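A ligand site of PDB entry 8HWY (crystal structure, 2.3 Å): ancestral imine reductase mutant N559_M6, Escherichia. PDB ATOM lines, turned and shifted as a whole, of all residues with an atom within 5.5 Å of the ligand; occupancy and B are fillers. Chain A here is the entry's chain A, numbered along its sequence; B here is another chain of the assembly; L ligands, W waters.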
ATOM      1  N   GLY A  19      17.880 -13.258  27.005  1.00  0.00           N
ATOM      2  CA  GLY A  19      19.193 -13.770  26.671  1.00  0.00           C
ATOM      3  C   GLY A  19      20.265 -13.133  27.537  1.00  0.00           C
ATOM      4  O   GLY A  19      20.510 -11.929  27.449  1.00  0.00           O
ATOM      5  N   LEU A  20      20.912 -13.920  28.386  1.00  0.00           N
ATOM      6  CA  LEU A  20      21.890 -13.400  29.324  1.00  0.00           C
ATOM      7  C   LEU A  20      23.272 -13.983  29.069  1.00  0.00           C
ATOM      8  O   LEU A  20      23.988 -14.375  29.987  1.00  0.00           O
ATOM      9  CB  LEU A  20      21.461 -13.674  30.753  1.00  0.00           C
ATOM     10  CG  LEU A  20      20.231 -12.872  31.151  1.00  0.00           C
ATOM     11  CD1 LEU A  20      19.868 -13.229  32.621  1.00  0.00           C
ATOM     12  CD2 LEU A  20      20.483 -11.356  30.967  1.00  0.00           C
ATOM     13  N   GLY A  21      23.669 -14.029  27.802  1.00  0.00           N
ATOM     14  CA  GLY A  21      25.061 -14.218  27.488  1.00  0.00           C
ATOM     15  C   GLY A  21      25.801 -13.009  28.000  1.00  0.00           C
ATOM     16  O   GLY A  21      25.191 -12.090  28.556  1.00  0.00           O
ATOM     17  N   PRO A  22      27.122 -12.942  27.792  1.00  0.00           N
ATOM     18  CA  PRO A  22      27.885 -11.781  28.314  1.00  0.00           C
ATOM     19  C   PRO A  22      27.346 -10.445  27.808  1.00  0.00           C
ATOM     20  O   PRO A  22      27.350  -9.462  28.577  1.00  0.00           O
ATOM     21  CB  PRO A  22      29.322 -12.045  27.814  1.00  0.00           C
ATOM     22  CG  PRO A  22      29.170 -13.011  26.709  1.00  0.00           C
ATOM     23  CD  PRO A  22      27.950 -13.835  26.963  1.00  0.00           C
ATOM     24  N   MET A  23      26.877 -10.380  26.551  1.00  0.00           N
ATOM     25  CA  MET A  23      26.307  -9.130  26.024  1.00  0.00           C
ATOM     26  C   MET A  23      24.959  -8.832  26.663  1.00  0.00           C
ATOM     27  O   MET A  23      24.693  -7.698  27.069  1.00  0.00           O
ATOM     28  CB  MET A  23      26.190  -9.207  24.496  1.00  0.00           C
ATOM     29  CG  MET A  23      25.638  -7.927  23.931  1.00  0.00           C
ATOM     30  SD  MET A  23      26.841  -6.538  24.169  1.00  0.00           S
ATOM     31  CE  MET A  23      28.433  -7.192  23.656  1.00  0.00           C
ATOM     32  N   TRP A  41      15.439 -12.511  31.455  1.00  0.00           N
ATOM     33  CA  TRP A  41      15.095 -13.911  31.280  1.00  0.00           C
ATOM     34  C   TRP A  41      16.189 -14.582  30.483  1.00  0.00           C
ATOM     35  O   TRP A  41      16.659 -14.037  29.477  1.00  0.00           O
ATOM     36  CB  TRP A  41      13.763 -14.091  30.546  1.00  0.00           C
ATOM     37  CG  TRP A  41      13.393 -15.528  30.382  1.00  0.00           C
ATOM     38  CD1 TRP A  41      12.608 -16.276  31.216  1.00  0.00           C
ATOM     39  CD2 TRP A  41      13.796 -16.406  29.315  1.00  0.00           C
ATOM     40  NE1 TRP A  41      12.483 -17.560  30.726  1.00  0.00           N
ATOM     41  CE2 TRP A  41      13.207 -17.674  29.570  1.00  0.00           C
ATOM     42  CE3 TRP A  41      14.585 -16.244  28.166  1.00  0.00           C
ATOM     43  CZ2 TRP A  41      13.406 -18.791  28.716  1.00  0.00           C
ATOM     44  CZ3 TRP A  41      14.776 -17.365  27.308  1.00  0.00           C
ATOM     45  CH2 TRP A  41      14.183 -18.619  27.590  1.00  0.00           C
ATOM     46  N   ASN A  42      16.560 -15.791  30.914  1.00  0.00           N
ATOM     47  CA  ASN A  42      17.465 -16.607  30.139  1.00  0.00           C
ATOM     48  C   ASN A  42      16.954 -18.039  30.092  1.00  0.00           C
ATOM     49  O   ASN A  42      16.337 -18.522  31.049  1.00  0.00           O
ATOM     50  CB  ASN A  42      18.881 -16.578  30.734  1.00  0.00           C
ATOM     51  CG  ASN A  42      19.902 -17.026  29.751  1.00  0.00           C
ATOM     52  OD1 ASN A  42      20.000 -16.477  28.628  1.00  0.00           O
ATOM     53  ND2 ASN A  42      20.677 -18.052  30.126  1.00  0.00           N
ATOM     54  N   ARG A  43      17.237 -18.759  28.999  1.00  0.00           N
ATOM     55  CA  ARG A  43      16.881 -20.176  28.947  1.00  0.00           C
ATOM     56  C   ARG A  43      17.594 -20.957  30.041  1.00  0.00           C
ATOM     57  O   ARG A  43      16.984 -21.799  30.719  1.00  0.00           O
ATOM     58  CB  ARG A  43      17.206 -20.766  27.573  1.00  0.00           C
ATOM     59  CG  ARG A  43      17.165 -22.296  27.532  1.00  0.00           C
ATOM     60  CD  ARG A  43      17.646 -22.818  26.163  1.00  0.00           C
ATOM     61  NE  ARG A  43      19.044 -22.495  25.924  1.00  0.00           N
ATOM     62  CZ  ARG A  43      19.709 -22.855  24.830  1.00  0.00           C
ATOM     63  NH1 ARG A  43      19.129 -23.565  23.873  1.00  0.00           N
ATOM     64  NH2 ARG A  43      20.983 -22.492  24.694  1.00  0.00           N
ATOM     65  N   THR A  44      18.903 -20.723  30.220  1.00  0.00           N
ATOM     66  CA  THR A  44      19.671 -21.397  31.261  1.00  0.00           C
ATOM     67  C   THR A  44      19.566 -20.622  32.561  1.00  0.00           C
ATOM     68  O   THR A  44      20.037 -19.473  32.626  1.00  0.00           O
ATOM     69  CB  THR A  44      21.145 -21.570  30.898  1.00  0.00           C
ATOM     70  OG1 THR A  44      21.276 -22.351  29.703  1.00  0.00           O
ATOM     71  CG2 THR A  44      21.891 -22.343  32.015  1.00  0.00           C
ATOM     72  N   LYS A  47      22.257 -17.307  35.648  1.00  0.00           N
ATOM     73  CA  LYS A  47      23.163 -16.325  35.100  1.00  0.00           C
ATOM     74  C   LYS A  47      22.764 -14.924  35.509  1.00  0.00           C
ATOM     75  O   LYS A  47      23.425 -13.966  35.105  1.00  0.00           O
ATOM     76  CB  LYS A  47      23.224 -16.453  33.592  1.00  0.00           C
ATOM     77  CG  LYS A  47      24.016 -17.665  33.125  1.00  0.00           C
ATOM     78  CD  LYS A  47      24.171 -17.679  31.601  1.00  0.00           C
ATOM     79  CE  LYS A  47      24.638 -19.071  31.103  1.00  0.00           C
ATOM     80  NZ  LYS A  47      25.335 -19.063  29.754  1.00  0.00           N
ATOM     81  N   SER A  75      18.940 -10.611  22.956  1.00  0.00           N
ATOM     82  CA  SER A  75      20.375 -10.773  22.654  1.00  0.00           C
ATOM     83  C   SER A  75      20.691 -12.258  22.778  1.00  0.00           C
ATOM     84  O   SER A  75      21.173 -12.742  23.814  1.00  0.00           O
ATOM     85  CB  SER A  75      21.211  -9.907  23.580  1.00  0.00           C
ATOM     86  OG  SER A  75      22.596 -10.158  23.439  1.00  0.00           O
ATOM     87  N   VAL A  76      20.373 -13.013  21.744  1.00  0.00           N
ATOM     88  CA  VAL A  76      20.613 -14.444  21.713  1.00  0.00           C
ATOM     89  C   VAL A  76      21.309 -14.778  20.414  1.00  0.00           C
ATOM     90  O   VAL A  76      21.473 -13.922  19.547  1.00  0.00           O
ATOM     91  CB  VAL A  76      19.305 -15.248  21.838  1.00  0.00           C
ATOM     92  CG1 VAL A  76      18.645 -14.964  23.171  1.00  0.00           C
ATOM     93  CG2 VAL A  76      18.387 -14.934  20.597  1.00  0.00           C
ATOM     94  N   THR A  77      21.645 -16.063  20.257  1.00  0.00           N
ATOM     95  CA  THR A  77      22.621 -16.493  19.257  1.00  0.00           C
ATOM     96  C   THR A  77      22.199 -16.126  17.844  1.00  0.00           C
ATOM     97  O   THR A  77      23.013 -15.605  17.061  1.00  0.00           O
ATOM     98  CB  THR A  77      22.856 -18.008  19.357  1.00  0.00           C
ATOM     99  OG1 THR A  77      23.584 -18.335  20.549  1.00  0.00           O
ATOM    100  CG2 THR A  77      23.612 -18.531  18.144  1.00  0.00           C
ATOM    101  N   ASP A  78      20.945 -16.383  17.470  1.00  0.00           N
ATOM    102  CA  ASP A  78      20.522 -16.128  16.091  1.00  0.00           C
ATOM    103  C   ASP A  78      18.995 -16.081  15.974  1.00  0.00           C
ATOM    104  O   ASP A  78      18.258 -16.216  16.948  1.00  0.00           O
ATOM    105  CB  ASP A  78      21.089 -17.202  15.136  1.00  0.00           C
ATOM    106  CG  ASP A  78      20.779 -18.657  15.573  1.00  0.00           C
ATOM    107  OD1 ASP A  78      19.779 -18.884  16.300  1.00  0.00           O
ATOM    108  OD2 ASP A  78      21.532 -19.598  15.206  1.00  0.00           O
ATOM    109  N   ALA A  81      17.074 -19.134  17.445  1.00  0.00           N
ATOM    110  CA  ALA A  81      16.931 -19.074  18.903  1.00  0.00           C
ATOM    111  C   ALA A  81      15.923 -18.004  19.294  1.00  0.00           C
ATOM    112  O   ALA A  81      15.147 -18.178  20.229  1.00  0.00           O
ATOM    113  CB  ALA A  81      18.278 -18.811  19.563  1.00  0.00           C
ATOM    114  N   ALA A  84      12.354 -19.458  18.620  1.00  0.00           N
ATOM    115  CA  ALA A  84      11.962 -20.498  19.582  1.00  0.00           C
ATOM    116  C   ALA A  84      11.721 -19.896  20.963  1.00  0.00           C
ATOM    117  O   ALA A  84      10.724 -20.215  21.620  1.00  0.00           O
ATOM    118  CB  ALA A  84      13.006 -21.596  19.670  1.00  0.00           C
ATOM    119  N   ILE A  85      12.591 -18.991  21.401  1.00  0.00           N
ATOM    120  CA  ILE A  85      12.357 -18.296  22.665  1.00  0.00           C
ATOM    121  C   ILE A  85      10.981 -17.635  22.685  1.00  0.00           C
ATOM    122  O   ILE A  85      10.217 -17.778  23.647  1.00  0.00           O
ATOM    123  CB  ILE A  85      13.460 -17.255  22.901  1.00  0.00           C
ATOM    124  CG1 ILE A  85      14.765 -17.952  23.215  1.00  0.00           C
ATOM    125  CG2 ILE A  85      13.048 -16.285  24.025  1.00  0.00           C
ATOM    126  CD1 ILE A  85      15.970 -16.933  23.248  1.00  0.00           C
ATOM    127  N   LEU A 101      19.099  -7.798  18.795  1.00  0.00           N
ATOM    128  CA  LEU A 101      20.526  -7.856  18.510  1.00  0.00           C
ATOM    129  C   LEU A 101      20.971  -9.256  18.126  1.00  0.00           C
ATOM    130  O   LEU A 101      22.142  -9.600  18.299  1.00  0.00           O
ATOM    131  CB  LEU A 101      21.323  -7.368  19.718  1.00  0.00           C
ATOM    132  CG  LEU A 101      21.075  -5.900  20.008  1.00  0.00           C
ATOM    133  CD1 LEU A 101      20.334  -5.691  21.321  1.00  0.00           C
ATOM    134  CD2 LEU A 101      22.403  -5.163  19.995  1.00  0.00           C
ATOM    135  N   SER A 102      20.064 -10.073  17.601  1.00  0.00           N
ATOM    136  CA  SER A 102      20.348 -11.476  17.336  1.00  0.00           C
ATOM    137  C   SER A 102      20.179 -11.850  15.864  1.00  0.00           C
ATOM    138  O   SER A 102      19.905 -13.027  15.565  1.00  0.00           O
ATOM    139  CB  SER A 102      19.425 -12.328  18.201  1.00  0.00           C
ATOM    140  OG  SER A 102      19.265 -11.727  19.471  1.00  0.00           O
ATOM    141  N   SER A 103      20.241 -10.889  14.943  1.00  0.00           N
ATOM    142  CA  SER A 103      20.037 -11.178  13.517  1.00  0.00           C
ATOM    143  C   SER A 103      21.352 -11.624  12.908  1.00  0.00           C
ATOM    144  O   SER A 103      22.338 -10.866  12.884  1.00  0.00           O
ATOM    145  CB  SER A 103      19.483  -9.954  12.783  1.00  0.00           C
ATOM    146  OG  SER A 103      18.093  -9.824  13.029  1.00  0.00           O
ATOM    147  N   ASP A 125      16.363  -3.458  14.525  1.00  0.00           N
ATOM    148  CA  ASP A 125      17.528  -4.327  14.551  1.00  0.00           C
ATOM    149  C   ASP A 125      18.683  -3.553  15.140  1.00  0.00           C
ATOM    150  O   ASP A 125      18.856  -2.373  14.864  1.00  0.00           O
ATOM    151  CB  ASP A 125      17.919  -4.877  13.178  1.00  0.00           C
ATOM    152  CG  ASP A 125      18.557  -6.303  13.273  1.00  0.00           C
ATOM    153  OD1 ASP A 125      17.829  -7.315  13.525  1.00  0.00           O
ATOM    154  OD2 ASP A 125      19.802  -6.397  13.156  1.00  0.00           O
ATOM    155  N   GLY A 126      19.466  -4.220  15.976  1.00  0.00           N
ATOM    156  CA  GLY A 126      20.562  -3.568  16.665  1.00  0.00           C
ATOM    157  C   GLY A 126      21.842  -4.333  16.498  1.00  0.00           C
ATOM    158  O   GLY A 126      21.852  -5.550  16.308  1.00  0.00           O
ATOM    159  N   GLY A 127      22.931  -3.601  16.571  1.00  0.00           N
ATOM    160  CA  GLY A 127      24.219  -4.226  16.440  1.00  0.00           C
ATOM    161  C   GLY A 127      25.250  -3.420  17.163  1.00  0.00           C
ATOM    162  O   GLY A 127      25.239  -2.185  17.125  1.00  0.00           O
ATOM    163  N   VAL A 128      26.163  -4.133  17.805  1.00  0.00           N
ATOM    164  CA  VAL A 128      27.237  -3.560  18.580  1.00  0.00           C
ATOM    165  C   VAL A 128      28.432  -4.493  18.476  1.00  0.00           C
ATOM    166  O   VAL A 128      28.298  -5.718  18.611  1.00  0.00           O
ATOM    167  CB  VAL A 128      26.818  -3.368  20.056  1.00  0.00           C
ATOM    168  CG1 VAL A 128      26.465  -4.711  20.672  1.00  0.00           C
ATOM    169  CG2 VAL A 128      27.922  -2.695  20.846  1.00  0.00           C
ATOM    170  N   VAL A 130      31.503  -4.265  20.452  1.00  0.00           N
ATOM    171  CA  VAL A 130      32.419  -3.805  21.504  1.00  0.00           C
ATOM    172  C   VAL A 130      32.471  -4.880  22.568  1.00  0.00           C
ATOM    173  O   VAL A 130      31.591  -5.752  22.643  1.00  0.00           O
ATOM    174  CB  VAL A 130      31.987  -2.450  22.109  1.00  0.00           C
ATOM    175  CG1 VAL A 130      32.132  -1.308  21.118  1.00  0.00           C
ATOM    176  CG2 VAL A 130      30.546  -2.536  22.644  1.00  0.00           C
ATOM    177  N   PRO A 132      31.840  -6.525  26.085  1.00  0.00           N
ATOM    178  CA  PRO A 132      30.718  -6.302  27.027  1.00  0.00           C
ATOM    179  C   PRO A 132      31.010  -5.234  28.069  1.00  0.00           C
ATOM    180  O   PRO A 132      30.148  -4.365  28.320  1.00  0.00           O
ATOM    181  CB  PRO A 132      30.536  -7.691  27.673  1.00  0.00           C
ATOM    182  CG  PRO A 132      30.852  -8.619  26.527  1.00  0.00           C
ATOM    183  CD  PRO A 132      31.988  -7.946  25.752  1.00  0.00           C
ATOM    184  N   ALA A 174      21.517  -2.822  10.174  1.00  0.00           N
ATOM    185  CA  ALA A 174      22.341  -3.081  11.354  1.00  0.00           C
ATOM    186  C   ALA A 174      22.991  -4.442  11.234  1.00  0.00           C
ATOM    187  O   ALA A 174      24.169  -4.608  11.548  1.00  0.00           O
ATOM    188  CB  ALA A 174      21.497  -2.998  12.631  1.00  0.00           C
ATOM    189  N   ALA A 175      22.234  -5.417  10.744  1.00  0.00           N
ATOM    190  CA  ALA A 175      22.803  -6.754  10.610  1.00  0.00           C
ATOM    191  C   ALA A 175      23.924  -6.742   9.596  1.00  0.00           C
ATOM    192  O   ALA A 175      24.925  -7.466   9.768  1.00  0.00           O
ATOM    193  CB  ALA A 175      21.725  -7.759  10.206  1.00  0.00           C
ATOM    194  N   TYR A 178      26.960  -5.409  11.151  1.00  0.00           N
ATOM    195  CA  TYR A 178      27.521  -6.317  12.138  1.00  0.00           C
ATOM    196  C   TYR A 178      28.327  -7.423  11.474  1.00  0.00           C
ATOM    197  O   TYR A 178      29.414  -7.751  11.942  1.00  0.00           O
ATOM    198  CB  TYR A 178      26.426  -6.928  13.039  1.00  0.00           C
ATOM    199  CG  TYR A 178      27.045  -7.836  14.077  1.00  0.00           C
ATOM    200  CD1 TYR A 178      27.666  -7.302  15.208  1.00  0.00           C
ATOM    201  CD2 TYR A 178      27.096  -9.216  13.888  1.00  0.00           C
ATOM    202  CE1 TYR A 178      28.284  -8.116  16.148  1.00  0.00           C
ATOM    203  CE2 TYR A 178      27.731 -10.045  14.828  1.00  0.00           C
ATOM    204  CZ  TYR A 178      28.321  -9.478  15.953  1.00  0.00           C
ATOM    205  OH  TYR A 178      28.960 -10.262  16.901  1.00  0.00           O
ATOM    206  N   GLU B 239      33.392 -18.081  27.256  1.00  0.00           N
ATOM    207  CA  GLU B 239      32.065 -17.847  26.703  1.00  0.00           C
ATOM    208  C   GLU B 239      32.084 -17.563  25.193  1.00  0.00           C
ATOM    209  O   GLU B 239      31.085 -17.076  24.659  1.00  0.00           O
ATOM    210  CB  GLU B 239      31.373 -16.723  27.486  1.00  0.00           C
ATOM    211  CG  GLU B 239      30.274 -17.259  28.394  1.00  0.00           C
ATOM    212  CD  GLU B 239      29.760 -16.241  29.430  1.00  0.00           C
ATOM    213  OE1 GLU B 239      30.579 -15.561  30.108  1.00  0.00           O
ATOM    214  OE2 GLU B 239      28.511 -16.138  29.550  1.00  0.00           O
ATOM    215  N   MET B 244      31.352 -21.726  18.103  1.00  0.00           N
ATOM    216  CA  MET B 244      30.482 -20.556  17.949  1.00  0.00           C
ATOM    217  C   MET B 244      31.079 -19.529  16.996  1.00  0.00           C
ATOM    218  O   MET B 244      30.348 -18.891  16.220  1.00  0.00           O
ATOM    219  CB  MET B 244      30.210 -19.892  19.302  1.00  0.00           C
ATOM    220  CG  MET B 244      29.744 -20.845  20.401  1.00  0.00           C
ATOM    221  SD  MET B 244      30.119 -20.165  22.034  1.00  0.00           S
ATOM    222  CE  MET B 244      29.401 -18.525  21.936  1.00  0.00           C
HETATM  223  P1  LIG L   1      26.423 -16.131  23.685  1.00  0.00           P
HETATM  224  O1  LIG L   1      27.302 -15.142  24.360  1.00  0.00           O
HETATM  225  O2  LIG L   1      26.583 -17.575  24.016  1.00  0.00           O
HETATM  226  O3  LIG L   1      24.893 -15.704  23.900  1.00  0.00           O
HETATM  227  C1  LIG L   1      23.864 -16.542  23.333  1.00  0.00           C
HETATM  228  C2  LIG L   1      22.594 -16.348  24.108  1.00  0.00           C
HETATM  229  O4  LIG L   1      21.504 -16.936  23.357  1.00  0.00           O
HETATM  230  C3  LIG L   1      22.547 -17.017  25.498  1.00  0.00           C
HETATM  231  O5  LIG L   1      21.861 -16.202  26.425  1.00  0.00           O
HETATM  232  C4  LIG L   1      21.807 -18.315  25.218  1.00  0.00           C
HETATM  233  O6  LIG L   1      21.103 -18.815  26.343  1.00  0.00           O
HETATM  234  C5  LIG L   1      20.811 -17.842  24.175  1.00  0.00           C
HETATM  235  N1  LIG L   1      20.293 -18.911  23.348  1.00  0.00           N
HETATM  236  C6  LIG L   1      20.918 -19.500  22.283  1.00  0.00           C
HETATM  237  N2  LIG L   1      20.202 -20.437  21.720  1.00  0.00           N
HETATM  238  C7  LIG L   1      19.032 -20.458  22.449  1.00  0.00           C
HETATM  239  C8  LIG L   1      17.859 -21.239  22.343  1.00  0.00           C
HETATM  240  N3  LIG L   1      17.688 -22.175  21.423  1.00  0.00           N
HETATM  241  N4  LIG L   1      16.881 -21.005  23.230  1.00  0.00           N
HETATM  242  C9  LIG L   1      17.058 -20.057  24.156  1.00  0.00           C
HETATM  243  N5  LIG L   1      18.113 -19.274  24.352  1.00  0.00           N
HETATM  244  C10 LIG L   1      19.065 -19.517  23.454  1.00  0.00           C
HETATM  245  O7  LIG L   1      26.589 -15.965  22.103  1.00  0.00           O
HETATM  246  P2  LIG L   1      25.900 -15.094  20.964  1.00  0.00           P
HETATM  247  O8  LIG L   1      24.871 -14.192  21.560  1.00  0.00           O
HETATM  248  O9  LIG L   1      25.477 -16.044  19.899  1.00  0.00           O
HETATM  249  O10 LIG L   1      27.130 -14.222  20.430  1.00  0.00           O
HETATM  250  C11 LIG L   1      28.069 -13.680  21.388  1.00  0.00           C
HETATM  251  C12 LIG L   1      28.574 -12.353  20.910  1.00  0.00           C
HETATM  252  O11 LIG L   1      28.118 -12.097  19.555  1.00  0.00           O
HETATM  253  C13 LIG L   1      28.119 -11.136  21.731  1.00  0.00           C
HETATM  254  O12 LIG L   1      29.157 -10.186  21.867  1.00  0.00           O
HETATM  255  C14 LIG L   1      26.948 -10.590  20.914  1.00  0.00           C
HETATM  256  O13 LIG L   1      26.716  -9.196  21.090  1.00  0.00           O
HETATM  257  C15 LIG L   1      27.479 -10.831  19.506  1.00  0.00           C
HETATM  258  N6  LIG L   1      26.415 -10.848  18.491  1.00  0.00           N
HETATM  259  C16 LIG L   1      25.909  -9.648  18.040  1.00  0.00           C
HETATM  260  C17 LIG L   1      24.909  -9.632  17.091  1.00  0.00           C
HETATM  261  C18 LIG L   1      24.386  -8.302  16.632  1.00  0.00           C
HETATM  262  O14 LIG L   1      23.793  -8.215  15.548  1.00  0.00           O
HETATM  263  N7  LIG L   1      24.564  -7.261  17.429  1.00  0.00           N
HETATM  264  C19 LIG L   1      24.404 -10.822  16.597  1.00  0.00           C
HETATM  265  C20 LIG L   1      24.908 -12.026  17.057  1.00  0.00           C
HETATM  266  C21 LIG L   1      25.915 -12.026  18.004  1.00  0.00           C
HETATM  267  P3  LIG L   1      21.840 -19.911  27.270  1.00  0.00           P
HETATM  268  O15 LIG L   1      22.507 -19.199  28.398  1.00  0.00           O
HETATM  269  O16 LIG L   1      20.676 -20.744  27.727  1.00  0.00           O
HETATM  270  O17 LIG L   1      22.826 -20.715  26.456  1.00  0.00           O
HETATM  271  O   HOH W   1      25.854 -15.219  17.461  1.00  0.00           O
HETATM  272  O   HOH W   2      30.444  -7.754  20.364  1.00  0.00           O
HETATM  273  O   HOH W   3      20.729  -7.942  15.061  1.00  0.00           O
HETATM  274  O   HOH W   4      26.317 -12.633  24.281  1.00  0.00           O
HETATM  275  O   HOH W   5      18.348 -17.600  26.605  1.00  0.00           O
HETATM  276  O   HOH W   6      14.179 -22.408  23.339  1.00  0.00           O
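OH of Tyr 178 sits close to O11 of the ligand (3.3 Å). O15 of the ligand is in hydrogen-bond range of ND2 of Asn 42 (2.8 Å). The side-chain hydroxyl (OG1) of Thr 77 sits close to an oxygen (O9) of the ligand (3.0 Å). OG1 of Thr 44 is in hydrogen-bond range of O16 of the ligand, 2.6 Å away. The guanidinium group (NE) of Arg 43 lies within salt-bridge range of an oxygen (O16) of the ligand (3.0 Å). N of Leu 20 lies within hydrogen-bond range of O5 of the ligand, at 3.2 Å. NZ of Lys 47 lies within salt-bridge range of O15 of the ligand. The backbone NH of Thr 77 is in hydrogen-bond range of an oxygen (O4) of the ligand (3.2 Å). O of Gly 126 sits at hydrogen-bond distance from N7 of the ligand, 3.4 Å away. O of Leu 101 sits close to N7 of the ligand (3.5 Å). The backbone NH of Thr 44 sits at hydrogen-bond distance from an oxygen (O16) of the ligand (3.1 Å). An oxygen (O5) of the ligand sits at hydrogen-bond distance from the backbone NH (N) of Gly 21.
The backbone carbonyl oxygen of Thr 44 sits at hydrogen-bond distance from the side-chain amide nitrogen of Asn 42. OD1 of Asp 78 sits at hydrogen-bond distance from N of Ala 81, at 2.9 Å. N of Leu 20 lies within hydrogen-bond range of OD1 of Asn 42 (2.7 Å). The backbone NH of Val 76 sits at hydrogen-bond distance from the side-chain hydroxyl of Ser 102 (2.8 Å). The backbone NH (N) of Gly 19 lies within hydrogen-bond range of the backbone carbonyl oxygen (O) of Trp 41, 2.9 Å away.
Gly 19 touches the ligand (CA to O5, 3.6 Å). Pro 22 touches the ligand (CD to O1, 3.0 Å). Met 23 touches the ligand. Ser 75 touches the ligand (O to C2, 3.9 Å). Val 76 touches the ligand (CA to O4, 3.1 Å). CB of Ala 81 touches N2 of the ligand, at 3.3 Å. Ile 85 touches the ligand (CG1 to C9, 3.3 Å). Gly 127 touches the ligand. Val 128 touches the ligand (N to N7, 3.5 Å). Met 244 of chain B touches the ligand. 20 residues have an atom within 4 Å of the ligand: Gly 19, Leu 20, Gly 21, Pro 22, Met 23, Asn 42, Arg 43, Thr 44, Lys 47, Ser 75, Val 76, Thr 77, Ala 81, Ile 85, Leu 101, Gly 126, Gly 127, Val 128, Tyr 178 and Met 244 of chain B. The nearest printed residue that does not touch the ligand is Ser 103 (4.03 Å).
Water W1 bridges an oxygen (O9) of the ligand (2.6 Å) and the backbone carbonyl oxygen of Thr 77 (2.9 Å). Water W4 bridges O1 of the ligand and N of Met 23. Water W5 lies within hydrogen-bond range of a nitrogen (N5) of the ligand (2.8 Å), the side-chain amide oxygen (OD1) of Asn 42 (2.8 Å) and the backbone NH (N) of Arg 43 (2.9 Å). Water W2 lies within hydrogen-bond range of an oxygen (O12) of the ligand (3.1 Å), the backbone carbonyl oxygen of Val 130 (3.2 Å) and the backbone carbonyl oxygen of Val 128 (3.4 Å).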
